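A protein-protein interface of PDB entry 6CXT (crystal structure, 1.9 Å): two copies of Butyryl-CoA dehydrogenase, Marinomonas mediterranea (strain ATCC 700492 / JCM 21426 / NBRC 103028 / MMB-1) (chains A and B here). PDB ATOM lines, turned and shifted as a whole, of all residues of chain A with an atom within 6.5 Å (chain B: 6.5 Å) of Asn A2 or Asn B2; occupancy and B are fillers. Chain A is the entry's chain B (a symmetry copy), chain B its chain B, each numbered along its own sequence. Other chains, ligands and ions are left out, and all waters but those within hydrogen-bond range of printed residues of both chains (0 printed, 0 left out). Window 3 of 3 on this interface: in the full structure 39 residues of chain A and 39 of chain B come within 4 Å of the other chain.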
ATOM      1  N   MET A   1      11.043  26.800   6.485  1.00  0.00           N
ATOM      2  CA  MET A   1      10.983  27.513   7.801  1.00  0.00           C
ATOM      3  C   MET A   1      10.250  26.677   8.845  1.00  0.00           C
ATOM      4  O   MET A   1       9.011  26.569   8.821  1.00  0.00           O
ATOM      5  CB  MET A   1      10.337  28.891   7.569  1.00  0.00           C
ATOM      6  CG  MET A   1       9.890  29.730   8.771  1.00  0.00           C
ATOM      7  SD  MET A   1      11.176  30.746   9.497  1.00  0.00           S
ATOM      8  CE  MET A   1      11.809  31.795   8.169  1.00  0.00           C
ATOM      9  N   ASN A   2      10.998  26.113   9.797  1.00  0.00           N
ATOM     10  CA  ASN A   2      10.385  25.386  10.908  1.00  0.00           C
ATOM     11  C   ASN A   2      11.283  25.450  12.147  1.00  0.00           C
ATOM     12  O   ASN A   2      12.480  25.710  12.023  1.00  0.00           O
ATOM     13  CB  ASN A   2      10.119  23.894  10.535  1.00  0.00           C
ATOM     14  CG  ASN A   2      11.393  23.089  10.463  1.00  0.00           C
ATOM     15  OD1 ASN A   2      11.858  22.538  11.470  1.00  0.00           O
ATOM     16  ND2 ASN A   2      12.026  23.101   9.295  1.00  0.00           N
ATOM     17  N   PHE A   3      10.707  25.157  13.310  1.00  0.00           N
ATOM     18  CA  PHE A   3      11.428  25.236  14.561  1.00  0.00           C
ATOM     19  C   PHE A   3      11.485  23.893  15.260  1.00  0.00           C
ATOM     20  O   PHE A   3      11.579  23.798  16.474  1.00  0.00           O
ATOM     21  CB  PHE A   3      10.807  26.317  15.443  1.00  0.00           C
ATOM     22  CG  PHE A   3      10.927  27.688  14.855  1.00  0.00           C
ATOM     23  CD1 PHE A   3       9.962  28.164  13.950  1.00  0.00           C
ATOM     24  CD2 PHE A   3      12.024  28.502  15.160  1.00  0.00           C
ATOM     25  CE1 PHE A   3      10.089  29.433  13.382  1.00  0.00           C
ATOM     26  CE2 PHE A   3      12.126  29.778  14.621  1.00  0.00           C
ATOM     27  CZ  PHE A   3      11.163  30.239  13.724  1.00  0.00           C
ATOM     28  N   GLU A   4      11.468  22.848  14.443  1.00  0.00           N
ATOM     29  CA  GLU A   4      11.400  21.472  14.918  1.00  0.00           C
ATOM     30  C   GLU A   4      12.832  20.925  15.047  1.00  0.00           C
ATOM     31  O   GLU A   4      13.658  21.111  14.152  1.00  0.00           O
ATOM     32  CB  GLU A   4      10.539  20.682  13.891  1.00  0.00           C
ATOM     33  CG  GLU A   4      10.339  19.191  14.110  1.00  0.00           C
ATOM     34  CD  GLU A   4       9.265  18.828  15.132  1.00  0.00           C
ATOM     35  OE1 GLU A   4       8.868  19.682  15.978  1.00  0.00           O
ATOM     36  OE2 GLU A   4       8.805  17.657  15.079  1.00  0.00           O
ATOM     37  N   TRP A   5      13.143  20.331  16.189  1.00  0.00           N
ATOM     38  CA  TRP A   5      14.432  19.619  16.362  1.00  0.00           C
ATOM     39  C   TRP A   5      14.206  18.157  15.968  1.00  0.00           C
ATOM     40  O   TRP A   5      13.149  17.624  16.280  1.00  0.00           O
ATOM     41  CB  TRP A   5      14.900  19.704  17.822  1.00  0.00           C
ATOM     42  CG  TRP A   5      15.281  21.127  18.191  1.00  0.00           C
ATOM     43  CD1 TRP A   5      14.521  22.046  18.892  1.00  0.00           C
ATOM     44  CD2 TRP A   5      16.501  21.785  17.852  1.00  0.00           C
ATOM     45  NE1 TRP A   5      15.213  23.243  18.995  1.00  0.00           N
ATOM     46  CE2 TRP A   5      16.426  23.114  18.373  1.00  0.00           C
ATOM     47  CE3 TRP A   5      17.653  21.395  17.155  1.00  0.00           C
ATOM     48  CZ2 TRP A   5      17.451  24.042  18.206  1.00  0.00           C
ATOM     49  CZ3 TRP A   5      18.705  22.324  17.016  1.00  0.00           C
ATOM     50  CH2 TRP A   5      18.582  23.636  17.536  1.00  0.00           C
ATOM     51  N   LEU A  65      23.970  24.056  14.341  1.00  0.00           N
ATOM     52  CA  LEU A  65      22.761  24.016  15.153  1.00  0.00           C
ATOM     53  C   LEU A  65      22.740  22.968  16.227  1.00  0.00           C
ATOM     54  O   LEU A  65      22.308  23.257  17.367  1.00  0.00           O
ATOM     55  CB  LEU A  65      21.476  23.892  14.309  1.00  0.00           C
ATOM     56  CG  LEU A  65      20.952  25.247  13.831  1.00  0.00           C
ATOM     57  CD1 LEU A  65      20.003  25.016  12.655  1.00  0.00           C
ATOM     58  CD2 LEU A  65      20.270  26.047  14.972  1.00  0.00           C
ATOM     59  N   TRP A 304      21.952  28.911  12.209  1.00  0.00           N
ATOM     60  CA  TRP A 304      21.468  28.450  10.910  1.00  0.00           C
ATOM     61  C   TRP A 304      22.114  29.222   9.782  1.00  0.00           C
ATOM     62  O   TRP A 304      22.513  28.640   8.765  1.00  0.00           O
ATOM     63  CB  TRP A 304      19.926  28.565  10.810  1.00  0.00           C
ATOM     64  CG  TRP A 304      19.427  28.258   9.431  1.00  0.00           C
ATOM     65  CD1 TRP A 304      19.145  27.021   8.925  1.00  0.00           C
ATOM     66  CD2 TRP A 304      19.168  29.194   8.392  1.00  0.00           C
ATOM     67  NE1 TRP A 304      18.717  27.132   7.620  1.00  0.00           N
ATOM     68  CE2 TRP A 304      18.719  28.451   7.264  1.00  0.00           C
ATOM     69  CE3 TRP A 304      19.242  30.590   8.301  1.00  0.00           C
ATOM     70  CZ2 TRP A 304      18.359  29.059   6.053  1.00  0.00           C
ATOM     71  CZ3 TRP A 304      18.883  31.199   7.078  1.00  0.00           C
ATOM     72  CH2 TRP A 304      18.438  30.421   5.979  1.00  0.00           C
ATOM     73  N   MET B   1      14.808  22.301  12.176  1.00  0.00           N
ATOM     74  CA  MET B   1      15.037  23.754  12.460  1.00  0.00           C
ATOM     75  C   MET B   1      15.759  24.432  11.300  1.00  0.00           C
ATOM     76  O   MET B   1      16.975  24.254  11.112  1.00  0.00           O
ATOM     77  CB  MET B   1      15.800  23.866  13.793  1.00  0.00           C
ATOM     78  CG  MET B   1      16.417  25.207  14.202  1.00  0.00           C
ATOM     79  SD  MET B   1      15.298  26.321  15.050  1.00  0.00           S
ATOM     80  CE  MET B   1      14.677  25.423  16.490  1.00  0.00           C
ATOM     81  N   ASN B   2      15.031  25.252  10.536  1.00  0.00           N
ATOM     82  CA  ASN B   2      15.648  26.037   9.469  1.00  0.00           C
ATOM     83  C   ASN B   2      14.856  27.326   9.229  1.00  0.00           C
ATOM     84  O   ASN B   2      13.685  27.404   9.603  1.00  0.00           O
ATOM     85  CB  ASN B   2      15.734  25.225   8.139  1.00  0.00           C
ATOM     86  CG  ASN B   2      14.384  25.052   7.489  1.00  0.00           C
ATOM     87  OD1 ASN B   2      13.942  25.900   6.701  1.00  0.00           O
ATOM     88  ND2 ASN B   2      13.670  24.008   7.894  1.00  0.00           N
ATOM     89  N   PHE B   3      15.484  28.291   8.563  1.00  0.00           N
ATOM     90  CA  PHE B   3      14.870  29.577   8.321  1.00  0.00           C
ATOM     91  C   PHE B   3      14.730  29.862   6.839  1.00  0.00           C
ATOM     92  O   PHE B   3      14.718  30.999   6.396  1.00  0.00           O
ATOM     93  CB  PHE B   3      15.661  30.667   9.042  1.00  0.00           C
ATOM     94  CG  PHE B   3      15.637  30.515  10.531  1.00  0.00           C
ATOM     95  CD1 PHE B   3      16.574  29.693  11.180  1.00  0.00           C
ATOM     96  CD2 PHE B   3      14.652  31.150  11.298  1.00  0.00           C
ATOM     97  CE1 PHE B   3      16.533  29.531  12.566  1.00  0.00           C
ATOM     98  CE2 PHE B   3      14.639  31.016  12.679  1.00  0.00           C
ATOM     99  CZ  PHE B   3      15.575  30.198  13.312  1.00  0.00           C
ATOM    100  N   GLU B   4      14.581  28.780   6.085  1.00  0.00           N
ATOM    101  CA  GLU B   4      14.545  28.828   4.630  1.00  0.00           C
ATOM    102  C   GLU B   4      13.079  28.938   4.177  1.00  0.00           C
ATOM    103  O   GLU B   4      12.211  28.222   4.680  1.00  0.00           O
ATOM    104  CB  GLU B   4      15.243  27.536   4.117  1.00  0.00           C
ATOM    105  CG  GLU B   4      15.308  27.294   2.618  1.00  0.00           C
ATOM    106  CD  GLU B   4      16.412  28.054   1.889  1.00  0.00           C
ATOM    107  OE1 GLU B   4      16.956  29.065   2.421  1.00  0.00           O
ATOM    108  OE2 GLU B   4      16.747  27.619   0.756  1.00  0.00           O
ATOM    109  N   TRP B   5      12.796  29.885   3.295  1.00  0.00           N
ATOM    110  CA  TRP B   5      11.458  29.974   2.662  1.00  0.00           C
ATOM    111  C   TRP B   5      11.505  29.154   1.370  1.00  0.00           C
ATOM    112  O   TRP B   5      12.524  29.191   0.692  1.00  0.00           O
ATOM    113  CB  TRP B   5      11.111  31.435   2.344  1.00  0.00           C
ATOM    114  CG  TRP B   5      10.903  32.237   3.619  1.00  0.00           C
ATOM    115  CD1 TRP B   5      11.802  33.092   4.230  1.00  0.00           C
ATOM    116  CD2 TRP B   5       9.734  32.227   4.437  1.00  0.00           C
ATOM    117  NE1 TRP B   5      11.243  33.605   5.390  1.00  0.00           N
ATOM    118  CE2 TRP B   5       9.982  33.098   5.542  1.00  0.00           C
ATOM    119  CE3 TRP B   5       8.500  31.566   4.359  1.00  0.00           C
ATOM    120  CZ2 TRP B   5       9.045  33.310   6.552  1.00  0.00           C
ATOM    121  CZ3 TRP B   5       7.540  31.807   5.362  1.00  0.00           C
ATOM    122  CH2 TRP B   5       7.833  32.669   6.448  1.00  0.00           C
ATOM    123  N   LEU B  65       2.292  30.291   8.197  1.00  0.00           N
ATOM    124  CA  LEU B  65       3.548  30.931   7.828  1.00  0.00           C
ATOM    125  C   LEU B  65       3.543  31.649   6.509  1.00  0.00           C
ATOM    126  O   LEU B  65       4.085  32.775   6.415  1.00  0.00           O
ATOM    127  CB  LEU B  65       4.747  29.962   7.863  1.00  0.00           C
ATOM    128  CG  LEU B  65       5.368  29.846   9.257  1.00  0.00           C
ATOM    129  CD1 LEU B  65       6.199  28.564   9.315  1.00  0.00           C
ATOM    130  CD2 LEU B  65       6.210  31.094   9.630  1.00  0.00           C
ATOM    131  N   TRP B 304       4.624  29.459  13.301  1.00  0.00           N
ATOM    132  CA  TRP B 304       4.961  28.041  13.211  1.00  0.00           C
ATOM    133  C   TRP B 304       4.314  27.254  14.328  1.00  0.00           C
ATOM    134  O   TRP B 304       3.784  26.158  14.106  1.00  0.00           O
ATOM    135  CB  TRP B 304       6.495  27.824  13.235  1.00  0.00           C
ATOM    136  CG  TRP B 304       6.856  26.371  13.314  1.00  0.00           C
ATOM    137  CD1 TRP B 304       6.975  25.504  12.266  1.00  0.00           C
ATOM    138  CD2 TRP B 304       7.130  25.626  14.494  1.00  0.00           C
ATOM    139  NE1 TRP B 304       7.312  24.251  12.727  1.00  0.00           N
ATOM    140  CE2 TRP B 304       7.418  24.293  14.089  1.00  0.00           C
ATOM    141  CE3 TRP B 304       7.191  25.951  15.857  1.00  0.00           C
ATOM    142  CZ2 TRP B 304       7.746  23.279  14.999  1.00  0.00           C
ATOM    143  CZ3 TRP B 304       7.517  24.925  16.772  1.00  0.00           C
ATOM    144  CH2 TRP B 304       7.798  23.609  16.324  1.00  0.00           C
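The backbone NH (N) of Met B1 sits at hydrogen-bond distance from the side-chain amide oxygen (OD1) of Asn A2, at 3.0 Å. OD1 of Asn B2 is in hydrogen-bond range of N of Met A1 (3.0 Å). The backbone NH of Asn B2 lies within hydrogen-bond range of the backbone carbonyl oxygen of Asn A2. N of Met B1 sits at hydrogen-bond distance from O of Glu A4. The backbone NH (N) of Met A1 sits at hydrogen-bond distance from the backbone carbonyl oxygen (O) of Glu B4, 2.6 Å away.
Of chain B, only Met B1, Asn B2 and Trp B304 come within 4 Å of Asn A2. Asn B2 touches three residues of chain A. Of the printed residues of chain B, Trp A5 touches Met B1. Of the printed residues of chain A, Glu B4 touches Met A1 (2.6 Å) and Trp A304 (3.8 Å). Of the printed residues of chain A, Met B1 touches Asn A2, Phe A3, Glu A4, Trp A5 and Leu A65. Of the printed residues of chain A, Phe B3 touches Met A1 (3.5 Å), Phe A3 (3.4 Å) and Trp A304 (3.5 Å). Of the printed residues of chain B, Phe A3 touches Met B1, Phe B3 and Trp B304. The nearest residue of chain B that does not touch Asn A2 is Phe B3 (5.1 Å). The nearest residue of chain A that does not touch Asn B2 is Phe A3 (5.1 Å). The nearest printed residue of chain A that does not touch Glu B4 is Asn A2 (5.7 Å).
CE of Met A1 touches O of Phe B3, 3.5 Å away. CE of Met A1 touches NE1 of Trp B5 (3.4 Å). Met A1 touches Leu B65 (O to CD1, 3.5 Å). Trp B304 touches Asn A2. Phe A3 touches Met B1. CE2 of Phe A3 touches CE2 of Phe B3, at 3.4 Å. N of Phe A3 touches CE2 of Trp B304 (3.5 Å). CB of Asn B2 touches NE1 of Trp A304, 3.6 Å away. Trp A304 touches Phe B3. CZ2 of Trp A304 touches N of Glu B4, at 3.8 Å.
Of the 7 printed residues of chain B, 7 touch a printed residue of chain A. Printed residues of chain B that touch a printed residue of chain A: Met B1, Asn B2, Phe B3, Glu B4, Trp B5, Leu B65 and Trp B304. Hydrophobic or aromatic side chains of chain B that line the printed part of chain A: Met B1, Phe B3, Trp B5, Leu B65 and Trp B304. Along chain A the printed residues that touch a printed residue of chain B span positions 1 to 304. Among the printed residues, 18 pairs touch across the chains. Among the printed residues, no Asp or Glu carboxylate lies within 4 Å of a Lys or Arg side-chain nitrogen of the other chain.
Met A1 touches Phe B3, and with the chains exchanged Phe A3 touches Met B1. Met A1 touches Leu B65, and with the chains exchanged Leu A65 touches Met B1. Asn A2 touches Trp B304, and with the chains exchanged Trp A304 touches Asn B2. Glu A4 touches Trp B304, and with the chains exchanged Trp A304 touches Glu B4. Of the 18 pairs that touch across the chains among the printed residues, 18 have their exchanged pair printed and touching as well.
The side-chain amide oxygen of Asn B2 lies within hydrogen-bond range of the backbone NH of Glu B4. The backbone NH of Glu A4 sits at hydrogen-bond distance from the side-chain amide oxygen of Asn A2 (3.0 Å).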
